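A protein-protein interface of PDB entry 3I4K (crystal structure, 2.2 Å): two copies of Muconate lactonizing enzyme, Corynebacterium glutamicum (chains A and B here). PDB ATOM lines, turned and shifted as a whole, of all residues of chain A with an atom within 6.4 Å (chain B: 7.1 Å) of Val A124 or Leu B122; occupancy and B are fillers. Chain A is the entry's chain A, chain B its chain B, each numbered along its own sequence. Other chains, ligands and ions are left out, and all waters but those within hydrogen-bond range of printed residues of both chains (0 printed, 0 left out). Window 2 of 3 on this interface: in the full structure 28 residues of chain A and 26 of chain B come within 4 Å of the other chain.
N of Val A124 is in hydrogen-bond range of O of Ala A119.
The backbone carbonyl oxygen of Val A124 is in hydrogen-bond range of the backbone NH of Gly A359 (3.0 Å).
The backbone carbonyl oxygen of Ala B119 lies within hydrogen-bond range of the backbone NH of Val B124, 2.9 Å away.
Of chain A, only Val A124 (3.7 Å) comes within 4 Å of Leu B122.
Printed residues of chain A within 4 Å of Trp B118: Asp A128 (3.4 Å).
Of the printed residues of chain A, Val B124 touches Leu A122 (3.96 Å).
Printed residues of chain B within 4 Å of Leu A122: Val B124 (3.96 Å).
Of the printed residues of chain B, Leu A129 touches Leu B129 (3.4 Å).
Asp B116 touches none of the printed residues of chain A.
Pro B125 touches none of the printed residues of chain A.
The nearest residue of chain B that does not touch Val A124 is Trp B118 (6.3 Å).
The nearest residue of chain A that does not touch Leu B122 is Leu A122 (5.2 Å).
The nearest printed residue of chain B that does not touch Leu A122 is Leu B122 (5.2 Å).
Leu A122 touches Val B124, and with the chains exchanged Val A124 touches Leu B122.
Leu A129 touches its own counterpart, Leu B129.
Positions printed for both chains: 116, 118, 119, 120, 121, 122, 123, 124, 125, 129 and 358.
Hydrophobic or aromatic side chains of chain B within 4 Å of the printed part of chain A: Trp B118, Leu B122, Val B124 and Leu B129.
Among the printed residues, no Asp or Glu carboxylate lies within 4 Å of a Lys or Arg side-chain nitrogen of the other chain.
O of Leu A129 sits close to O of Leu B129 (3.4 Å).
Among the printed residues, merely in contact across the chains: Asp A128 with Leu B129 (3.2 Å), Asp A128 with Trp B118 (3.4 Å), Val A124 with Leu B122 (3.7 Å) and Leu A122 with Val B124 (3.96 Å).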
ATOM      1  N   ASP A 116      18.514   4.065 -18.041  1.00  0.00           N
ATOM      2  CA  ASP A 116      18.272   2.651 -17.767  1.00  0.00           C
ATOM      3  C   ASP A 116      16.950   2.483 -17.001  1.00  0.00           C
ATOM      4  O   ASP A 116      16.054   1.770 -17.443  1.00  0.00           O
ATOM      5  CB  ASP A 116      19.453   2.075 -16.966  1.00  0.00           C
ATOM      6  CG  ASP A 116      19.472   0.548 -16.938  1.00  0.00           C
ATOM      7  OD1 ASP A 116      19.077  -0.093 -17.939  1.00  0.00           O
ATOM      8  OD2 ASP A 116      19.918  -0.012 -15.914  1.00  0.00           O
ATOM      9  N   TRP A 118      14.431   4.358 -16.745  1.00  0.00           N
ATOM     10  CA  TRP A 118      13.281   4.752 -17.559  1.00  0.00           C
ATOM     11  C   TRP A 118      12.971   3.737 -18.669  1.00  0.00           C
ATOM     12  O   TRP A 118      11.815   3.356 -18.868  1.00  0.00           O
ATOM     13  CB  TRP A 118      13.540   6.139 -18.158  1.00  0.00           C
ATOM     14  CG  TRP A 118      12.313   6.877 -18.619  1.00  0.00           C
ATOM     15  CD1 TRP A 118      11.012   6.586 -18.319  1.00  0.00           C
ATOM     16  CD2 TRP A 118      12.283   8.070 -19.411  1.00  0.00           C
ATOM     17  NE1 TRP A 118      10.174   7.525 -18.872  1.00  0.00           N
ATOM     18  CE2 TRP A 118      10.929   8.448 -19.547  1.00  0.00           C
ATOM     19  CE3 TRP A 118      13.272   8.858 -20.017  1.00  0.00           C
ATOM     20  CZ2 TRP A 118      10.537   9.581 -20.266  1.00  0.00           C
ATOM     21  CZ3 TRP A 118      12.883   9.983 -20.731  1.00  0.00           C
ATOM     22  CH2 TRP A 118      11.526  10.334 -20.849  1.00  0.00           C
ATOM     23  N   ALA A 119      13.999   3.296 -19.388  1.00  0.00           N
ATOM     24  CA  ALA A 119      13.806   2.332 -20.464  1.00  0.00           C
ATOM     25  C   ALA A 119      13.256   1.000 -19.936  1.00  0.00           C
ATOM     26  O   ALA A 119      12.455   0.344 -20.603  1.00  0.00           O
ATOM     27  CB  ALA A 119      15.115   2.107 -21.207  1.00  0.00           C
ATOM     28  N   ARG A 120      13.696   0.592 -18.750  1.00  0.00           N
ATOM     29  CA  ARG A 120      13.209  -0.656 -18.165  1.00  0.00           C
ATOM     30  C   ARG A 120      11.767  -0.472 -17.696  1.00  0.00           C
ATOM     31  O   ARG A 120      10.935  -1.370 -17.855  1.00  0.00           O
ATOM     32  CB  ARG A 120      14.106  -1.093 -16.999  1.00  0.00           C
ATOM     33  CG  ARG A 120      15.443  -1.680 -17.448  1.00  0.00           C
ATOM     34  CD  ARG A 120      16.356  -1.976 -16.270  1.00  0.00           C
ATOM     35  NE  ARG A 120      17.642  -2.515 -16.699  1.00  0.00           N
ATOM     36  CZ  ARG A 120      17.817  -3.743 -17.175  1.00  0.00           C
ATOM     37  NH1 ARG A 120      16.783  -4.570 -17.279  1.00  0.00           N
ATOM     38  NH2 ARG A 120      19.019  -4.137 -17.573  1.00  0.00           N
ATOM     39  N   SER A 121      11.475   0.700 -17.134  1.00  0.00           N
ATOM     40  CA  SER A 121      10.133   1.009 -16.662  1.00  0.00           C
ATOM     41  C   SER A 121       9.132   1.001 -17.810  1.00  0.00           C
ATOM     42  O   SER A 121       7.961   0.674 -17.616  1.00  0.00           O
ATOM     43  CB  SER A 121      10.094   2.383 -15.986  1.00  0.00           C
ATOM     44  OG  SER A 121      10.726   2.367 -14.720  1.00  0.00           O
ATOM     45  N   LEU A 122       9.591   1.370 -19.003  1.00  0.00           N
ATOM     46  CA  LEU A 122       8.722   1.409 -20.178  1.00  0.00           C
ATOM     47  C   LEU A 122       8.832   0.093 -20.926  1.00  0.00           C
ATOM     48  O   LEU A 122       8.143  -0.141 -21.923  1.00  0.00           O
ATOM     49  CB  LEU A 122       9.132   2.555 -21.104  1.00  0.00           C
ATOM     50  CG  LEU A 122       9.198   3.975 -20.538  1.00  0.00           C
ATOM     51  CD1 LEU A 122       9.668   4.920 -21.648  1.00  0.00           C
ATOM     52  CD2 LEU A 122       7.837   4.413 -20.000  1.00  0.00           C
ATOM     53  N   ASN A 123       9.721  -0.759 -20.430  1.00  0.00           N
ATOM     54  CA  ASN A 123       9.972  -2.069 -21.010  1.00  0.00           C
ATOM     55  C   ASN A 123      10.511  -2.003 -22.439  1.00  0.00           C
ATOM     56  O   ASN A 123       9.999  -2.662 -23.351  1.00  0.00           O
ATOM     57  CB  ASN A 123       8.700  -2.926 -20.955  1.00  0.00           C
ATOM     58  CG  ASN A 123       8.985  -4.396 -21.198  1.00  0.00           C
ATOM     59  OD1 ASN A 123       9.801  -5.008 -20.501  1.00  0.00           O
ATOM     60  ND2 ASN A 123       8.318  -4.974 -22.193  1.00  0.00           N
ATOM     61  N   VAL A 124      11.564  -1.210 -22.623  1.00  0.00           N
ATOM     62  CA  VAL A 124      12.202  -1.059 -23.928  1.00  0.00           C
ATOM     63  C   VAL A 124      13.709  -0.910 -23.752  1.00  0.00           C
ATOM     64  O   VAL A 124      14.187  -0.649 -22.649  1.00  0.00           O
ATOM     65  CB  VAL A 124      11.692   0.203 -24.658  1.00  0.00           C
ATOM     66  CG1 VAL A 124      10.208   0.098 -24.917  1.00  0.00           C
ATOM     67  CG2 VAL A 124      12.003   1.441 -23.826  1.00  0.00           C
ATOM     68  N   PRO A 125      14.481  -1.091 -24.837  1.00  0.00           N
ATOM     69  CA  PRO A 125      15.940  -0.951 -24.759  1.00  0.00           C
ATOM     70  C   PRO A 125      16.231   0.534 -24.517  1.00  0.00           C
ATOM     71  O   PRO A 125      15.363   1.379 -24.750  1.00  0.00           O
ATOM     72  CB  PRO A 125      16.408  -1.377 -26.150  1.00  0.00           C
ATOM     73  CG  PRO A 125      15.286  -2.237 -26.666  1.00  0.00           C
ATOM     74  CD  PRO A 125      14.066  -1.531 -26.178  1.00  0.00           C
ATOM     75  N   VAL A 126      17.430   0.864 -24.055  1.00  0.00           N
ATOM     76  CA  VAL A 126      17.761   2.267 -23.836  1.00  0.00           C
ATOM     77  C   VAL A 126      17.799   3.032 -25.167  1.00  0.00           C
ATOM     78  O   VAL A 126      17.496   4.225 -25.211  1.00  0.00           O
ATOM     79  CB  VAL A 126      19.120   2.409 -23.124  1.00  0.00           C
ATOM     80  CG1 VAL A 126      19.749   3.751 -23.454  1.00  0.00           C
ATOM     81  CG2 VAL A 126      18.928   2.282 -21.611  1.00  0.00           C
ATOM     82  N   ARG A 127      18.158   2.343 -26.248  1.00  0.00           N
ATOM     83  CA  ARG A 127      18.244   2.969 -27.569  1.00  0.00           C
ATOM     84  C   ARG A 127      16.903   3.471 -28.106  1.00  0.00           C
ATOM     85  O   ARG A 127      16.865   4.352 -28.963  1.00  0.00           O
ATOM     86  CB  ARG A 127      18.835   1.993 -28.581  1.00  0.00           C
ATOM     87  CG  ARG A 127      18.013   0.734 -28.740  1.00  0.00           C
ATOM     88  CD  ARG A 127      18.584  -0.179 -29.788  1.00  0.00           C
ATOM     89  NE  ARG A 127      17.762  -1.370 -29.946  1.00  0.00           N
ATOM     90  CZ  ARG A 127      17.729  -2.370 -29.073  1.00  0.00           C
ATOM     91  NH1 ARG A 127      18.483  -2.322 -27.983  1.00  0.00           N
ATOM     92  NH2 ARG A 127      16.932  -3.410 -29.286  1.00  0.00           N
ATOM     93  N   ASP A 128      15.806   2.901 -27.627  1.00  0.00           N
ATOM     94  CA  ASP A 128      14.495   3.338 -28.087  1.00  0.00           C
ATOM     95  C   ASP A 128      14.138   4.692 -27.476  1.00  0.00           C
ATOM     96  O   ASP A 128      13.100   5.266 -27.787  1.00  0.00           O
ATOM     97  CB  ASP A 128      13.421   2.302 -27.749  1.00  0.00           C
ATOM     98  CG  ASP A 128      13.492   1.073 -28.637  1.00  0.00           C
ATOM     99  OD1 ASP A 128      14.259   1.070 -29.629  1.00  0.00           O
ATOM    100  OD2 ASP A 128      12.764   0.107 -28.342  1.00  0.00           O
ATOM    101  N   LEU A 129      14.991   5.196 -26.591  1.00  0.00           N
ATOM    102  CA  LEU A 129      14.754   6.507 -26.004  1.00  0.00           C
ATOM    103  C   LEU A 129      15.693   7.467 -26.726  1.00  0.00           C
ATOM    104  O   LEU A 129      15.655   8.683 -26.511  1.00  0.00           O
ATOM    105  CB  LEU A 129      15.073   6.512 -24.508  1.00  0.00           C
ATOM    106  CG  LEU A 129      14.240   5.624 -23.579  1.00  0.00           C
ATOM    107  CD1 LEU A 129      14.611   5.919 -22.136  1.00  0.00           C
ATOM    108  CD2 LEU A 129      12.767   5.884 -23.805  1.00  0.00           C
ATOM    109  N   GLY A 357      17.251  -6.484 -25.358  1.00  0.00           N
ATOM    110  CA  GLY A 357      16.550  -6.563 -24.091  1.00  0.00           C
ATOM    111  C   GLY A 357      16.318  -5.193 -23.484  1.00  0.00           C
ATOM    112  O   GLY A 357      16.890  -4.200 -23.938  1.00  0.00           O
ATOM    113  N   PRO A 358      15.488  -5.113 -22.437  1.00  0.00           N
ATOM    114  CA  PRO A 358      15.170  -3.855 -21.756  1.00  0.00           C
ATOM    115  C   PRO A 358      16.400  -3.153 -21.183  1.00  0.00           C
ATOM    116  O   PRO A 358      17.460  -3.766 -21.029  1.00  0.00           O
ATOM    117  CB  PRO A 358      14.196  -4.299 -20.668  1.00  0.00           C
ATOM    118  CG  PRO A 358      14.702  -5.666 -20.324  1.00  0.00           C
ATOM    119  CD  PRO A 358      14.944  -6.260 -21.691  1.00  0.00           C
ATOM    120  N   GLY A 359      16.245  -1.870 -20.861  1.00  0.00           N
ATOM    121  CA  GLY A 359      17.348  -1.106 -20.304  1.00  0.00           C
ATOM    122  C   GLY A 359      18.585  -1.196 -21.175  1.00  0.00           C
ATOM    123  O   GLY A 359      18.474  -1.169 -22.402  1.00  0.00           O
ATOM    124  N   LEU A 360      19.760  -1.311 -20.557  1.00  0.00           N
ATOM    125  CA  LEU A 360      20.996  -1.410 -21.327  1.00  0.00           C
ATOM    126  C   LEU A 360      21.073  -2.732 -22.078  1.00  0.00           C
ATOM    127  O   LEU A 360      21.919  -2.906 -22.954  1.00  0.00           O
ATOM    128  CB  LEU A 360      22.228  -1.277 -20.422  1.00  0.00           C
ATOM    129  CG  LEU A 360      22.666   0.088 -19.880  1.00  0.00           C
ATOM    130  CD1 LEU A 360      22.381   1.172 -20.906  1.00  0.00           C
ATOM    131  CD2 LEU A 360      21.945   0.385 -18.598  1.00  0.00           C
ATOM    132  N   LEU B   6       5.036  -3.822 -34.604  1.00  0.00           N
ATOM    133  CA  LEU B   6       5.368  -2.405 -34.647  1.00  0.00           C
ATOM    134  C   LEU B   6       5.628  -2.118 -36.122  1.00  0.00           C
ATOM    135  O   LEU B   6       5.935  -0.993 -36.516  1.00  0.00           O
ATOM    136  CB  LEU B   6       6.628  -2.143 -33.816  1.00  0.00           C
ATOM    137  CG  LEU B   6       6.580  -1.051 -32.749  1.00  0.00           C
ATOM    138  CD1 LEU B   6       5.324  -1.170 -31.904  1.00  0.00           C
ATOM    139  CD2 LEU B   6       7.830  -1.165 -31.885  1.00  0.00           C
ATOM    140  N   ASN B  45      -0.091  -3.396 -35.106  1.00  0.00           N
ATOM    141  CA  ASN B  45      -0.930  -3.373 -33.916  1.00  0.00           C
ATOM    142  C   ASN B  45      -2.154  -2.458 -34.017  1.00  0.00           C
ATOM    143  O   ASN B  45      -2.860  -2.254 -33.029  1.00  0.00           O
ATOM    144  CB  ASN B  45      -0.082  -2.948 -32.720  1.00  0.00           C
ATOM    145  CG  ASN B  45       0.608  -1.612 -32.941  1.00  0.00           C
ATOM    146  OD1 ASN B  45       1.382  -1.155 -32.102  1.00  0.00           O
ATOM    147  ND2 ASN B  45       0.327  -0.980 -34.075  1.00  0.00           N
ATOM    148  N   VAL B  47      -2.273   0.802 -34.335  1.00  0.00           N
ATOM    149  CA  VAL B  47      -2.082   2.191 -33.920  1.00  0.00           C
ATOM    150  C   VAL B  47      -1.715   3.029 -35.144  1.00  0.00           C
ATOM    151  O   VAL B  47      -1.050   2.543 -36.061  1.00  0.00           O
ATOM    152  CB  VAL B  47      -0.965   2.322 -32.858  1.00  0.00           C
ATOM    153  CG1 VAL B  47       0.356   1.846 -33.432  1.00  0.00           C
ATOM    154  CG2 VAL B  47      -0.852   3.770 -32.390  1.00  0.00           C
ATOM    155  N   ASP B 116       4.875   9.720 -33.511  1.00  0.00           N
ATOM    156  CA  ASP B 116       3.525   9.682 -32.966  1.00  0.00           C
ATOM    157  C   ASP B 116       3.074   8.234 -32.803  1.00  0.00           C
ATOM    158  O   ASP B 116       2.683   7.815 -31.710  1.00  0.00           O
ATOM    159  CB  ASP B 116       2.578  10.438 -33.904  1.00  0.00           C
ATOM    160  CG  ASP B 116       1.170  10.555 -33.354  1.00  0.00           C
ATOM    161  OD1 ASP B 116       1.010  10.776 -32.133  1.00  0.00           O
ATOM    162  OD2 ASP B 116       0.221  10.451 -34.158  1.00  0.00           O
ATOM    163  N   ALA B 117       3.146   7.477 -33.894  1.00  0.00           N
ATOM    164  CA  ALA B 117       2.742   6.075 -33.900  1.00  0.00           C
ATOM    165  C   ALA B 117       3.559   5.267 -32.899  1.00  0.00           C
ATOM    166  O   ALA B 117       3.015   4.439 -32.156  1.00  0.00           O
ATOM    167  CB  ALA B 117       2.910   5.491 -35.302  1.00  0.00           C
ATOM    168  N   TRP B 118       4.868   5.518 -32.877  1.00  0.00           N
ATOM    169  CA  TRP B 118       5.754   4.801 -31.978  1.00  0.00           C
ATOM    170  C   TRP B 118       5.447   5.117 -30.522  1.00  0.00           C
ATOM    171  O   TRP B 118       5.325   4.201 -29.713  1.00  0.00           O
ATOM    172  CB  TRP B 118       7.224   5.121 -32.286  1.00  0.00           C
ATOM    173  CG  TRP B 118       8.193   4.140 -31.665  1.00  0.00           C
ATOM    174  CD1 TRP B 118       7.897   2.899 -31.176  1.00  0.00           C
ATOM    175  CD2 TRP B 118       9.616   4.293 -31.531  1.00  0.00           C
ATOM    176  NE1 TRP B 118       9.041   2.268 -30.748  1.00  0.00           N
ATOM    177  CE2 TRP B 118      10.111   3.099 -30.953  1.00  0.00           C
ATOM    178  CE3 TRP B 118      10.518   5.318 -31.843  1.00  0.00           C
ATOM    179  CZ2 TRP B 118      11.474   2.902 -30.682  1.00  0.00           C
ATOM    180  CZ3 TRP B 118      11.877   5.120 -31.574  1.00  0.00           C
ATOM    181  CH2 TRP B 118      12.337   3.921 -30.999  1.00  0.00           C
ATOM    182  N   ALA B 119       5.316   6.399 -30.188  1.00  0.00           N
ATOM    183  CA  ALA B 119       5.028   6.800 -28.809  1.00  0.00           C
ATOM    184  C   ALA B 119       3.691   6.252 -28.309  1.00  0.00           C
ATOM    185  O   ALA B 119       3.545   5.935 -27.124  1.00  0.00           O
ATOM    186  CB  ALA B 119       5.043   8.323 -28.683  1.00  0.00           C
ATOM    187  N   ARG B 120       2.716   6.162 -29.212  1.00  0.00           N
ATOM    188  CA  ARG B 120       1.398   5.648 -28.864  1.00  0.00           C
ATOM    189  C   ARG B 120       1.472   4.171 -28.500  1.00  0.00           C
ATOM    190  O   ARG B 120       0.870   3.740 -27.515  1.00  0.00           O
ATOM    191  CB  ARG B 120       0.420   5.854 -30.026  1.00  0.00           C
ATOM    192  CG  ARG B 120      -0.029   7.296 -30.187  1.00  0.00           C
ATOM    193  CD  ARG B 120      -0.929   7.492 -31.398  1.00  0.00           C
ATOM    194  NE  ARG B 120      -1.337   8.890 -31.528  1.00  0.00           N
ATOM    195  CZ  ARG B 120      -2.008   9.556 -30.593  1.00  0.00           C
ATOM    196  NH1 ARG B 120      -2.349   8.945 -29.467  1.00  0.00           N
ATOM    197  NH2 ARG B 120      -2.332  10.832 -30.779  1.00  0.00           N
ATOM    198  N   SER B 121       2.221   3.409 -29.289  1.00  0.00           N
ATOM    199  CA  SER B 121       2.390   1.979 -29.060  1.00  0.00           C
ATOM    200  C   SER B 121       3.060   1.696 -27.720  1.00  0.00           C
ATOM    201  O   SER B 121       2.886   0.620 -27.140  1.00  0.00           O
ATOM    202  CB  SER B 121       3.235   1.367 -30.174  1.00  0.00           C
ATOM    203  OG  SER B 121       2.654   1.607 -31.437  1.00  0.00           O
ATOM    204  N   LEU B 122       3.831   2.658 -27.235  1.00  0.00           N
ATOM    205  CA  LEU B 122       4.535   2.502 -25.971  1.00  0.00           C
ATOM    206  C   LEU B 122       3.756   3.246 -24.902  1.00  0.00           C
ATOM    207  O   LEU B 122       4.140   3.269 -23.732  1.00  0.00           O
ATOM    208  CB  LEU B 122       5.950   3.075 -26.084  1.00  0.00           C
ATOM    209  CG  LEU B 122       6.869   2.510 -27.173  1.00  0.00           C
ATOM    210  CD1 LEU B 122       8.131   3.349 -27.235  1.00  0.00           C
ATOM    211  CD2 LEU B 122       7.214   1.057 -26.881  1.00  0.00           C
ATOM    212  N   ASN B 123       2.665   3.872 -25.329  1.00  0.00           N
ATOM    213  CA  ASN B 123       1.791   4.628 -24.440  1.00  0.00           C
ATOM    214  C   ASN B 123       2.512   5.726 -23.652  1.00  0.00           C
ATOM    215  O   ASN B 123       2.450   5.766 -22.425  1.00  0.00           O
ATOM    216  CB  ASN B 123       1.069   3.671 -23.479  1.00  0.00           C
ATOM    217  CG  ASN B 123       0.029   4.372 -22.620  1.00  0.00           C
ATOM    218  OD1 ASN B 123      -0.942   4.936 -23.126  1.00  0.00           O
ATOM    219  ND2 ASN B 123       0.233   4.340 -21.308  1.00  0.00           N
ATOM    220  N   VAL B 124       3.197   6.615 -24.371  1.00  0.00           N
ATOM    221  CA  VAL B 124       3.905   7.737 -23.757  1.00  0.00           C
ATOM    222  C   VAL B 124       3.793   8.948 -24.675  1.00  0.00           C
ATOM    223  O   VAL B 124       3.374   8.829 -25.825  1.00  0.00           O
ATOM    224  CB  VAL B 124       5.420   7.444 -23.568  1.00  0.00           C
ATOM    225  CG1 VAL B 124       5.621   6.172 -22.764  1.00  0.00           C
ATOM    226  CG2 VAL B 124       6.109   7.348 -24.927  1.00  0.00           C
ATOM    227  N   PRO B 125       4.142  10.136 -24.169  1.00  0.00           N
ATOM    228  CA  PRO B 125       4.070  11.337 -25.007  1.00  0.00           C
ATOM    229  C   PRO B 125       5.246  11.277 -25.983  1.00  0.00           C
ATOM    230  O   PRO B 125       6.196  10.525 -25.767  1.00  0.00           O
ATOM    231  CB  PRO B 125       4.223  12.472 -24.003  1.00  0.00           C
ATOM    232  CG  PRO B 125       3.728  11.869 -22.713  1.00  0.00           C
ATOM    233  CD  PRO B 125       4.318  10.495 -22.754  1.00  0.00           C
ATOM    234  N   LEU B 129      10.313  10.363 -26.126  1.00  0.00           N
ATOM    235  CA  LEU B 129      11.211   9.678 -27.051  1.00  0.00           C
ATOM    236  C   LEU B 129      12.329  10.672 -27.386  1.00  0.00           C
ATOM    237  O   LEU B 129      13.248  10.362 -28.151  1.00  0.00           O
ATOM    238  CB  LEU B 129      10.477   9.298 -28.336  1.00  0.00           C
ATOM    239  CG  LEU B 129       9.508   8.114 -28.315  1.00  0.00           C
ATOM    240  CD1 LEU B 129       8.788   8.027 -29.647  1.00  0.00           C
ATOM    241  CD2 LEU B 129      10.282   6.821 -28.038  1.00  0.00           C
ATOM    242  N   PRO B 358      -0.543  10.388 -24.634  1.00  0.00           N
ATOM    243  CA  PRO B 358       0.262   9.643 -25.610  1.00  0.00           C
ATOM    244  C   PRO B 358       0.364  10.317 -26.981  1.00  0.00           C
ATOM    245  O   PRO B 358      -0.475  11.150 -27.337  1.00  0.00           O
ATOM    246  CB  PRO B 358      -0.444   8.286 -25.672  1.00  0.00           C
ATOM    247  CG  PRO B 358      -1.866   8.635 -25.385  1.00  0.00           C
ATOM    248  CD  PRO B 358      -1.723   9.605 -24.232  1.00  0.00           C
